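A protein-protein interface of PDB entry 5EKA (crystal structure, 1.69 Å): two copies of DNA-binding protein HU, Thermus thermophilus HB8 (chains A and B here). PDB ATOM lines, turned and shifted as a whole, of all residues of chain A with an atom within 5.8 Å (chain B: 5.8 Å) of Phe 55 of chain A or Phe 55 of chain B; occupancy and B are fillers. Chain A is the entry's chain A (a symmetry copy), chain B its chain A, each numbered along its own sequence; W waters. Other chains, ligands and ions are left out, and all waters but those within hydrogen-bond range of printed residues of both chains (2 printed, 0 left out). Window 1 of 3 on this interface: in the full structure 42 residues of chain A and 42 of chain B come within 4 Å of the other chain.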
ATOM      1  N   VAL A  37      18.747 -11.757  30.542  1.00  0.00           N
ATOM      2  CA  VAL A  37      17.780 -12.790  30.153  1.00  0.00           C
ATOM      3  C   VAL A  37      18.382 -14.130  30.574  1.00  0.00           C
ATOM      4  O   VAL A  37      17.691 -14.910  31.193  1.00  0.00           O
ATOM      5  CB  VAL A  37      17.383 -12.713  28.667  1.00  0.00           C
ATOM      6  CG1 VAL A  37      16.549 -13.933  28.234  1.00  0.00           C
ATOM      7  CG2 VAL A  37      16.651 -11.382  28.429  1.00  0.00           C
ATOM      8  N   LEU A  41      16.717 -16.880  33.258  1.00  0.00           N
ATOM      9  CA  LEU A  41      16.454 -18.266  32.902  1.00  0.00           C
ATOM     10  C   LEU A  41      17.232 -19.280  33.759  1.00  0.00           C
ATOM     11  O   LEU A  41      16.691 -20.314  34.166  1.00  0.00           O
ATOM     12  CB  LEU A  41      16.707 -18.482  31.414  1.00  0.00           C
ATOM     13  CG  LEU A  41      15.719 -17.766  30.484  1.00  0.00           C
ATOM     14  CD1 LEU A  41      16.204 -17.856  29.058  1.00  0.00           C
ATOM     15  CD2 LEU A  41      14.299 -18.301  30.622  1.00  0.00           C
ATOM     16  N   SER A  45      13.314 -18.320  36.240  1.00  0.00           N
ATOM     17  CA  SER A  45      12.311 -17.288  35.925  1.00  0.00           C
ATOM     18  C   SER A  45      11.732 -17.529  34.523  1.00  0.00           C
ATOM     19  O   SER A  45      12.425 -18.063  33.628  1.00  0.00           O
ATOM     20  CB  SER A  45      12.938 -15.886  35.996  1.00  0.00           C
ATOM     21  OG  SER A  45      13.376 -15.588  37.333  1.00  0.00           O
ATOM     22  N   LYS A  46      10.465 -17.140  34.337  1.00  0.00           N
ATOM     23  CA  LYS A  46       9.921 -16.907  32.994  1.00  0.00           C
ATOM     24  C   LYS A  46      10.333 -15.475  32.613  1.00  0.00           C
ATOM     25  O   LYS A  46      10.322 -14.600  33.468  1.00  0.00           O
ATOM     26  CB  LYS A  46       8.395 -17.003  33.004  1.00  0.00           C
ATOM     27  CG  LYS A  46       7.806 -18.251  33.629  1.00  0.00           C
ATOM     28  CD  LYS A  46       8.036 -19.518  32.818  1.00  0.00           C
ATOM     29  CE  LYS A  46       7.601 -20.773  33.592  1.00  0.00           C
ATOM     30  NZ  LYS A  46       8.621 -21.387  34.490  1.00  0.00           N
ATOM     31  N   VAL A  47      10.666 -15.240  31.347  1.00  0.00           N
ATOM     32  CA  VAL A  47      11.026 -13.931  30.879  1.00  0.00           C
ATOM     33  C   VAL A  47       9.952 -13.586  29.853  1.00  0.00           C
ATOM     34  O   VAL A  47       9.948 -14.108  28.751  1.00  0.00           O
ATOM     35  CB  VAL A  47      12.431 -13.874  30.263  1.00  0.00           C
ATOM     36  CG1 VAL A  47      12.673 -12.512  29.690  1.00  0.00           C
ATOM     37  CG2 VAL A  47      13.485 -14.207  31.301  1.00  0.00           C
ATOM     38  N   GLN A  48       9.087 -12.661  30.224  1.00  0.00           N
ATOM     39  CA  GLN A  48       7.935 -12.307  29.434  1.00  0.00           C
ATOM     40  C   GLN A  48       8.220 -10.966  28.746  1.00  0.00           C
ATOM     41  O   GLN A  48       8.519  -9.975  29.411  1.00  0.00           O
ATOM     42  CB  GLN A  48       6.715 -12.186  30.373  1.00  0.00           C
ATOM     43  CG  GLN A  48       5.457 -11.655  29.718  1.00  0.00           C
ATOM     44  CD  GLN A  48       4.739 -10.712  30.672  1.00  0.00           C
ATOM     45  OE1 GLN A  48       4.644  -9.412  30.309  1.00  0.00           O
ATOM     46  NE2 GLN A  48       4.322 -11.139  31.756  1.00  0.00           N
ATOM     47  N   LEU A  49       8.145 -10.940  27.424  1.00  0.00           N
ATOM     48  CA  LEU A  49       8.404  -9.719  26.652  1.00  0.00           C
ATOM     49  C   LEU A  49       7.093  -9.433  25.939  1.00  0.00           C
ATOM     50  O   LEU A  49       6.809  -9.977  24.877  1.00  0.00           O
ATOM     51  CB  LEU A  49       9.562  -9.902  25.680  1.00  0.00           C
ATOM     52  CG  LEU A  49      10.905 -10.307  26.274  1.00  0.00           C
ATOM     53  CD1 LEU A  49      11.945 -10.476  25.197  1.00  0.00           C
ATOM     54  CD2 LEU A  49      11.316  -9.211  27.250  1.00  0.00           C
ATOM     55  N   PHE A  52       6.038  -9.674  22.130  1.00  0.00           N
ATOM     56  CA  PHE A  52       7.113 -10.387  21.428  1.00  0.00           C
ATOM     57  C   PHE A  52       7.036 -11.894  21.714  1.00  0.00           C
ATOM     58  O   PHE A  52       6.667 -12.678  20.848  1.00  0.00           O
ATOM     59  CB  PHE A  52       8.482  -9.779  21.760  1.00  0.00           C
ATOM     60  CG  PHE A  52       9.628 -10.422  21.029  1.00  0.00           C
ATOM     61  CD1 PHE A  52       9.852 -10.143  19.699  1.00  0.00           C
ATOM     62  CD2 PHE A  52      10.458 -11.325  21.670  1.00  0.00           C
ATOM     63  CE1 PHE A  52      10.907 -10.717  19.005  1.00  0.00           C
ATOM     64  CE2 PHE A  52      11.533 -11.905  20.999  1.00  0.00           C
ATOM     65  CZ  PHE A  52      11.750 -11.610  19.656  1.00  0.00           C
ATOM     66  N   GLY A  53       7.285 -12.288  22.952  1.00  0.00           N
ATOM     67  CA  GLY A  53       7.141 -13.686  23.333  1.00  0.00           C
ATOM     68  C   GLY A  53       7.717 -13.951  24.711  1.00  0.00           C
ATOM     69  O   GLY A  53       8.121 -13.029  25.403  1.00  0.00           O
ATOM     70  N   THR A  54       7.692 -15.207  25.123  1.00  0.00           N
ATOM     71  CA  THR A  54       8.174 -15.564  26.458  1.00  0.00           C
ATOM     72  C   THR A  54       9.263 -16.617  26.375  1.00  0.00           C
ATOM     73  O   THR A  54       9.094 -17.639  25.693  1.00  0.00           O
ATOM     74  CB  THR A  54       7.003 -16.068  27.296  1.00  0.00           C
ATOM     75  OG1 THR A  54       5.981 -15.039  27.315  1.00  0.00           O
ATOM     76  CG2 THR A  54       7.390 -16.455  28.710  1.00  0.00           C
ATOM     77  N   PHE A  55      10.340 -16.387  27.125  1.00  0.00           N
ATOM     78  CA  PHE A  55      11.329 -17.435  27.339  1.00  0.00           C
ATOM     79  C   PHE A  55      11.060 -18.153  28.666  1.00  0.00           C
ATOM     80  O   PHE A  55      10.657 -17.550  29.667  1.00  0.00           O
ATOM     81  CB  PHE A  55      12.734 -16.847  27.377  1.00  0.00           C
ATOM     82  CG  PHE A  55      13.160 -16.159  26.120  1.00  0.00           C
ATOM     83  CD1 PHE A  55      13.797 -16.863  25.116  1.00  0.00           C
ATOM     84  CD2 PHE A  55      12.960 -14.773  25.952  1.00  0.00           C
ATOM     85  CE1 PHE A  55      14.263 -16.226  23.979  1.00  0.00           C
ATOM     86  CE2 PHE A  55      13.420 -14.161  24.807  1.00  0.00           C
ATOM     87  CZ  PHE A  55      14.033 -14.891  23.817  1.00  0.00           C
ATOM     88  N   GLU A  56      11.329 -19.444  28.682  1.00  0.00           N
ATOM     89  CA  GLU A  56      11.123 -20.211  29.887  1.00  0.00           C
ATOM     90  C   GLU A  56      12.031 -21.432  29.849  1.00  0.00           C
ATOM     91  O   GLU A  56      12.546 -21.799  28.816  1.00  0.00           O
ATOM     92  CB  GLU A  56       9.659 -20.652  29.978  1.00  0.00           C
ATOM     93  CG  GLU A  56       9.226 -21.704  28.941  1.00  0.00           C
ATOM     94  CD  GLU A  56       7.711 -21.892  28.864  1.00  0.00           C
ATOM     95  OE1 GLU A  56       6.971 -21.272  29.682  1.00  0.00           O
ATOM     96  OE2 GLU A  56       7.266 -22.676  27.980  1.00  0.00           O
ATOM     97  N   VAL A  57      12.239 -22.021  31.007  1.00  0.00           N
ATOM     98  CA  VAL A  57      12.961 -23.286  31.110  1.00  0.00           C
ATOM     99  C   VAL A  57      11.964 -24.416  31.141  1.00  0.00           C
ATOM    100  O   VAL A  57      11.089 -24.467  32.028  1.00  0.00           O
ATOM    101  CB  VAL A  57      13.800 -23.301  32.398  1.00  0.00           C
ATOM    102  CG1 VAL A  57      14.500 -24.652  32.573  1.00  0.00           C
ATOM    103  CG2 VAL A  57      14.793 -22.165  32.356  1.00  0.00           C
ATOM    104  N   ALA A  83      13.506 -22.444  26.209  1.00  0.00           N
ATOM    105  CA  ALA A  83      12.604 -22.425  25.085  1.00  0.00           C
ATOM    106  C   ALA A  83      11.969 -21.042  24.967  1.00  0.00           C
ATOM    107  O   ALA A  83      11.919 -20.284  25.942  1.00  0.00           O
ATOM    108  CB  ALA A  83      11.541 -23.474  25.243  1.00  0.00           C
ATOM    109  N   PHE A  84      11.470 -20.755  23.775  1.00  0.00           N
ATOM    110  CA  PHE A  84      10.770 -19.487  23.484  1.00  0.00           C
ATOM    111  C   PHE A  84       9.401 -19.788  22.918  1.00  0.00           C
ATOM    112  O   PHE A  84       9.259 -20.648  22.052  1.00  0.00           O
ATOM    113  CB  PHE A  84      11.581 -18.719  22.478  1.00  0.00           C
ATOM    114  CG  PHE A  84      10.940 -17.470  21.992  1.00  0.00           C
ATOM    115  CD1 PHE A  84      10.865 -16.341  22.803  1.00  0.00           C
ATOM    116  CD2 PHE A  84      10.497 -17.402  20.691  1.00  0.00           C
ATOM    117  CE1 PHE A  84      10.312 -15.178  22.318  1.00  0.00           C
ATOM    118  CE2 PHE A  84       9.949 -16.232  20.190  1.00  0.00           C
ATOM    119  CZ  PHE A  84       9.829 -15.132  21.008  1.00  0.00           C
ATOM    120  N   LYS A  85       8.394 -19.098  23.466  1.00  0.00           N
ATOM    121  CA  LYS A  85       7.024 -19.209  23.005  1.00  0.00           C
ATOM    122  C   LYS A  85       6.676 -17.864  22.351  1.00  0.00           C
ATOM    123  O   LYS A  85       6.494 -16.854  23.061  1.00  0.00           O
ATOM    124  CB  LYS A  85       6.089 -19.460  24.180  1.00  0.00           C
ATOM    125  CG  LYS A  85       4.649 -19.547  23.717  1.00  0.00           C
ATOM    126  CD  LYS A  85       3.843 -20.520  24.525  1.00  0.00           C
ATOM    127  CE  LYS A  85       2.596 -20.930  23.757  1.00  0.00           C
ATOM    128  NZ  LYS A  85       1.744 -19.767  23.372  1.00  0.00           N
ATOM    129  N   VAL B  37      13.900  -7.055  15.377  1.00  0.00           N
ATOM    130  CA  VAL B  37      13.924  -8.521  15.294  1.00  0.00           C
ATOM    131  C   VAL B  37      12.660  -8.934  14.540  1.00  0.00           C
ATOM    132  O   VAL B  37      12.759  -9.721  13.624  1.00  0.00           O
ATOM    133  CB  VAL B  37      14.093  -9.199  16.665  1.00  0.00           C
ATOM    134  CG1 VAL B  37      13.893 -10.723  16.578  1.00  0.00           C
ATOM    135  CG2 VAL B  37      15.473  -8.816  17.228  1.00  0.00           C
ATOM    136  N   LEU B  41      12.487 -11.055  10.934  1.00  0.00           N
ATOM    137  CA  LEU B  41      11.754 -12.305  10.791  1.00  0.00           C
ATOM    138  C   LEU B  41      10.619 -12.238   9.754  1.00  0.00           C
ATOM    139  O   LEU B  41      10.417 -13.175   8.974  1.00  0.00           O
ATOM    140  CB  LEU B  41      11.244 -12.771  12.149  1.00  0.00           C
ATOM    141  CG  LEU B  41      12.340 -13.204  13.133  1.00  0.00           C
ATOM    142  CD1 LEU B  41      11.741 -13.414  14.502  1.00  0.00           C
ATOM    143  CD2 LEU B  41      13.090 -14.443  12.659  1.00  0.00           C
ATOM    144  N   SER B  45      14.506 -13.281   7.257  1.00  0.00           N
ATOM    145  CA  SER B  45      15.889 -13.304   7.763  1.00  0.00           C
ATOM    146  C   SER B  45      16.004 -14.294   8.932  1.00  0.00           C
ATOM    147  O   SER B  45      15.028 -14.511   9.685  1.00  0.00           O
ATOM    148  CB  SER B  45      16.320 -11.903   8.223  1.00  0.00           C
ATOM    149  OG  SER B  45      16.342 -10.985   7.117  1.00  0.00           O
ATOM    150  N   LYS B  46      17.191 -14.894   9.078  1.00  0.00           N
ATOM    151  CA  LYS B  46      17.589 -15.512  10.348  1.00  0.00           C
ATOM    152  C   LYS B  46      18.148 -14.372  11.217  1.00  0.00           C
ATOM    153  O   LYS B  46      18.821 -13.495  10.693  1.00  0.00           O
ATOM    154  CB  LYS B  46      18.686 -16.554  10.123  1.00  0.00           C
ATOM    155  CG  LYS B  46      18.409 -17.601   9.063  1.00  0.00           C
ATOM    156  CD  LYS B  46      17.326 -18.597   9.445  1.00  0.00           C
ATOM    157  CE  LYS B  46      16.945 -19.503   8.263  1.00  0.00           C
ATOM    158  NZ  LYS B  46      15.887 -18.988   7.346  1.00  0.00           N
ATOM    159  N   VAL B  47      17.893 -14.403  12.522  1.00  0.00           N
ATOM    160  CA  VAL B  47      18.403 -13.409  13.425  1.00  0.00           C
ATOM    161  C   VAL B  47      19.313 -14.187  14.370  1.00  0.00           C
ATOM    162  O   VAL B  47      18.848 -14.908  15.236  1.00  0.00           O
ATOM    163  CB  VAL B  47      17.298 -12.668  14.193  1.00  0.00           C
ATOM    164  CG1 VAL B  47      17.917 -11.747  15.197  1.00  0.00           C
ATOM    165  CG2 VAL B  47      16.412 -11.891  13.239  1.00  0.00           C
ATOM    166  N   GLN B  48      20.606 -13.977  14.213  1.00  0.00           N
ATOM    167  CA  GLN B  48      21.611 -14.722  14.929  1.00  0.00           C
ATOM    168  C   GLN B  48      22.170 -13.825  16.041  1.00  0.00           C
ATOM    169  O   GLN B  48      22.659 -12.729  15.771  1.00  0.00           O
ATOM    170  CB  GLN B  48      22.727 -15.117  13.938  1.00  0.00           C
ATOM    171  CG  GLN B  48      23.942 -15.763  14.572  1.00  0.00           C
ATOM    172  CD  GLN B  48      25.206 -15.259  13.892  1.00  0.00           C
ATOM    173  OE1 GLN B  48      26.067 -14.530  14.638  1.00  0.00           O
ATOM    174  NE2 GLN B  48      25.380 -15.475  12.685  1.00  0.00           N
ATOM    175  N   LEU B  49      22.083 -14.281  17.282  1.00  0.00           N
ATOM    176  CA  LEU B  49      22.576 -13.511  18.431  1.00  0.00           C
ATOM    177  C   LEU B  49      23.666 -14.380  19.033  1.00  0.00           C
ATOM    178  O   LEU B  49      23.404 -15.283  19.822  1.00  0.00           O
ATOM    179  CB  LEU B  49      21.462 -13.209  19.426  1.00  0.00           C
ATOM    180  CG  LEU B  49      20.257 -12.440  18.900  1.00  0.00           C
ATOM    181  CD1 LEU B  49      19.230 -12.238  19.984  1.00  0.00           C
ATOM    182  CD2 LEU B  49      20.766 -11.098  18.386  1.00  0.00           C
ATOM    183  N   PHE B  52      23.849 -16.449  22.405  1.00  0.00           N
ATOM    184  CA  PHE B  52      22.492 -16.483  22.965  1.00  0.00           C
ATOM    185  C   PHE B  52      21.620 -17.491  22.203  1.00  0.00           C
ATOM    186  O   PHE B  52      21.293 -18.553  22.719  1.00  0.00           O
ATOM    187  CB  PHE B  52      21.885 -15.075  23.015  1.00  0.00           C
ATOM    188  CG  PHE B  52      20.515 -15.024  23.634  1.00  0.00           C
ATOM    189  CD1 PHE B  52      20.362 -15.114  25.000  1.00  0.00           C
ATOM    190  CD2 PHE B  52      19.384 -14.916  22.843  1.00  0.00           C
ATOM    191  CE1 PHE B  52      19.111 -15.061  25.595  1.00  0.00           C
ATOM    192  CE2 PHE B  52      18.117 -14.848  23.416  1.00  0.00           C
ATOM    193  CZ  PHE B  52      17.979 -14.934  24.799  1.00  0.00           C
ATOM    194  N   GLY B  53      21.329 -17.208  20.945  1.00  0.00           N
ATOM    195  CA  GLY B  53      20.589 -18.153  20.119  1.00  0.00           C
ATOM    196  C   GLY B  53      20.150 -17.526  18.810  1.00  0.00           C
ATOM    197  O   GLY B  53      20.518 -16.402  18.505  1.00  0.00           O
ATOM    198  N   THR B  54      19.414 -18.285  18.016  1.00  0.00           N
ATOM    199  CA  THR B  54      18.982 -17.797  16.706  1.00  0.00           C
ATOM    200  C   THR B  54      17.472 -17.860  16.578  1.00  0.00           C
ATOM    201  O   THR B  54      16.862 -18.900  16.869  1.00  0.00           O
ATOM    202  CB  THR B  54      19.648 -18.629  15.615  1.00  0.00           C
ATOM    203  OG1 THR B  54      21.084 -18.559  15.804  1.00  0.00           O
ATOM    204  CG2 THR B  54      19.278 -18.196  14.210  1.00  0.00           C
ATOM    205  N   PHE B  55      16.893 -16.768  16.079  1.00  0.00           N
ATOM    206  CA  PHE B  55      15.498 -16.797  15.660  1.00  0.00           C
ATOM    207  C   PHE B  55      15.403 -17.043  14.150  1.00  0.00           C
ATOM    208  O   PHE B  55      16.216 -16.559  13.355  1.00  0.00           O
ATOM    209  CB  PHE B  55      14.814 -15.475  15.984  1.00  0.00           C
ATOM    210  CG  PHE B  55      14.779 -15.125  17.437  1.00  0.00           C
ATOM    211  CD1 PHE B  55      13.724 -15.531  18.231  1.00  0.00           C
ATOM    212  CD2 PHE B  55      15.799 -14.341  18.017  1.00  0.00           C
ATOM    213  CE1 PHE B  55      13.640 -15.154  19.560  1.00  0.00           C
ATOM    214  CE2 PHE B  55      15.703 -13.988  19.344  1.00  0.00           C
ATOM    215  CZ  PHE B  55      14.650 -14.422  20.114  1.00  0.00           C
ATOM    216  N   GLU B  56      14.374 -17.766  13.753  1.00  0.00           N
ATOM    217  CA  GLU B  56      14.185 -18.046  12.350  1.00  0.00           C
ATOM    218  C   GLU B  56      12.710 -18.328  12.103  1.00  0.00           C
ATOM    219  O   GLU B  56      11.959 -18.585  13.018  1.00  0.00           O
ATOM    220  CB  GLU B  56      15.024 -19.261  11.945  1.00  0.00           C
ATOM    221  CG  GLU B  56      14.552 -20.606  12.528  1.00  0.00           C
ATOM    222  CD  GLU B  56      15.571 -21.732  12.357  1.00  0.00           C
ATOM    223  OE1 GLU B  56      16.629 -21.511  11.698  1.00  0.00           O
ATOM    224  OE2 GLU B  56      15.299 -22.849  12.880  1.00  0.00           O
ATOM    225  N   VAL B  57      12.315 -18.232  10.852  1.00  0.00           N
ATOM    226  CA  VAL B  57      10.970 -18.619  10.436  1.00  0.00           C
ATOM    227  C   VAL B  57      11.006 -20.035   9.923  1.00  0.00           C
ATOM    228  O   VAL B  57      11.744 -20.347   8.967  1.00  0.00           O
ATOM    229  CB  VAL B  57      10.480 -17.678   9.323  1.00  0.00           C
ATOM    230  CG1 VAL B  57       9.106 -18.115   8.809  1.00  0.00           C
ATOM    231  CG2 VAL B  57      10.450 -16.263   9.848  1.00  0.00           C
ATOM    232  N   ALA B  83      10.501 -19.258  15.375  1.00  0.00           N
ATOM    233  CA  ALA B  83      11.061 -20.184  16.328  1.00  0.00           C
ATOM    234  C   ALA B  83      12.414 -19.665  16.806  1.00  0.00           C
ATOM    235  O   ALA B  83      13.056 -18.855  16.128  1.00  0.00           O
ATOM    236  CB  ALA B  83      11.214 -21.546  15.713  1.00  0.00           C
ATOM    237  N   PHE B  84      12.832 -20.167  17.957  1.00  0.00           N
ATOM    238  CA  PHE B  84      14.140 -19.825  18.553  1.00  0.00           C
ATOM    239  C   PHE B  84      14.916 -21.094  18.822  1.00  0.00           C
ATOM    240  O   PHE B  84      14.368 -22.063  19.341  1.00  0.00           O
ATOM    241  CB  PHE B  84      13.895 -19.093  19.842  1.00  0.00           C
ATOM    242  CG  PHE B  84      15.122 -18.789  20.623  1.00  0.00           C
ATOM    243  CD1 PHE B  84      16.001 -17.789  20.215  1.00  0.00           C
ATOM    244  CD2 PHE B  84      15.344 -19.444  21.813  1.00  0.00           C
ATOM    245  CE1 PHE B  84      17.106 -17.488  20.977  1.00  0.00           C
ATOM    246  CE2 PHE B  84      16.448 -19.140  22.594  1.00  0.00           C
ATOM    247  CZ  PHE B  84      17.343 -18.187  22.164  1.00  0.00           C
ATOM    248  N   LYS B  85      16.188 -21.082  18.406  1.00  0.00           N
ATOM    249  CA  LYS B  85      17.099 -22.185  18.637  1.00  0.00           C
ATOM    250  C   LYS B  85      18.145 -21.680  19.642  1.00  0.00           C
ATOM    251  O   LYS B  85      19.017 -20.864  19.278  1.00  0.00           O
ATOM    252  CB  LYS B  85      17.791 -22.581  17.340  1.00  0.00           C
ATOM    253  CG  LYS B  85      18.770 -23.713  17.572  1.00  0.00           C
ATOM    254  CD  LYS B  85      18.856 -24.648  16.403  1.00  0.00           C
ATOM    255  CE  LYS B  85      19.446 -25.980  16.841  1.00  0.00           C
ATOM    256  NZ  LYS B  85      20.790 -25.839  17.472  1.00  0.00           N
HETATM  257  O   HOH W   1      10.510 -21.301  19.465  1.00  0.00           O
HETATM  258  O   HOH W   2      12.687 -22.549  21.713  1.00  0.00           O
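Of the printed residues of chain B, Val 37 of chain A touches Phe 52 (3.8 Å). Of the printed residues of chain B, Phe 55 of chain A touches Phe 55 and Phe 84. Of the printed residues of chain A, Val 37 of chain B touches Phe 52 (3.8 Å). Of the printed residues of chain A, Phe 55 of chain B touches Phe 55 and Phe 84. Of the printed residues of chain A, Phe 84 of chain B touches Phe 55 (3.9 Å) and Phe 84 (3.5 Å). The nearest printed residue of chain B that does not touch Phe 55 of chain A is Phe 52 of chain B (4.02 Å). The nearest printed residue of chain A that does not touch Phe 55 of chain B is Phe 52 of chain A (4.02 Å).
Val 37 of chain A touches Phe 52 of chain B (CG1 to CE1, 3.8 Å). Val 37 of chain B touches Phe 52 of chain A. Phe 55 of chain B touches Phe 55 of chain A (CZ to CZ, 3.8 Å). CE1 of Phe 55 of chain A touches CE2 of Phe 84 of chain B, 3.9 Å away. CE2 of Phe 84 of chain A touches CE1 of Phe 55 of chain B, 3.9 Å away. Phe 84 of chain B touches Phe 84 of chain A (CB to CB, 3.5 Å).
Water W2 lies within hydrogen-bond range of O of Phe 84 of chain B (2.9 Å) and N of Phe 84 of chain A (3.0 Å). Water W1 bridges O of Phe 84 of chain A and N of Phe 84 of chain B.
O of Val 47 of chain B lies within hydrogen-bond range of N of Phe 55 of chain B. The backbone carbonyl oxygen (O) of Val 47 of chain A lies within hydrogen-bond range of the backbone NH (N) of Phe 55 of chain A (2.8 Å).
Hydrophobic or aromatic side chains of chain B that line the printed part of chain A: Val 37, Phe 52, Phe 55 and Phe 84. Of the 16 printed residues of chain A, 4 touch a printed residue of chain B. Among the printed residues, no Asp or Glu carboxylate lies within 4 Å of a Lys or Arg side-chain nitrogen of the other chain.
Val 37 of chain A touches Phe 52 of chain B, and with the chains exchanged Phe 52 of chain A touches Val 37 of chain B. Phe 55 of chain B touches its own counterpart, Phe 55 of chain A. Phe 55 of chain A touches Phe 84 of chain B, and with the chains exchanged Phe 84 of chain A touches Phe 55 of chain B. Phe 84 of chain B touches its own counterpart, Phe 84 of chain A. Of the 6 pairs that touch across the chains among the printed residues, 6 have their exchanged pair printed and touching as well.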
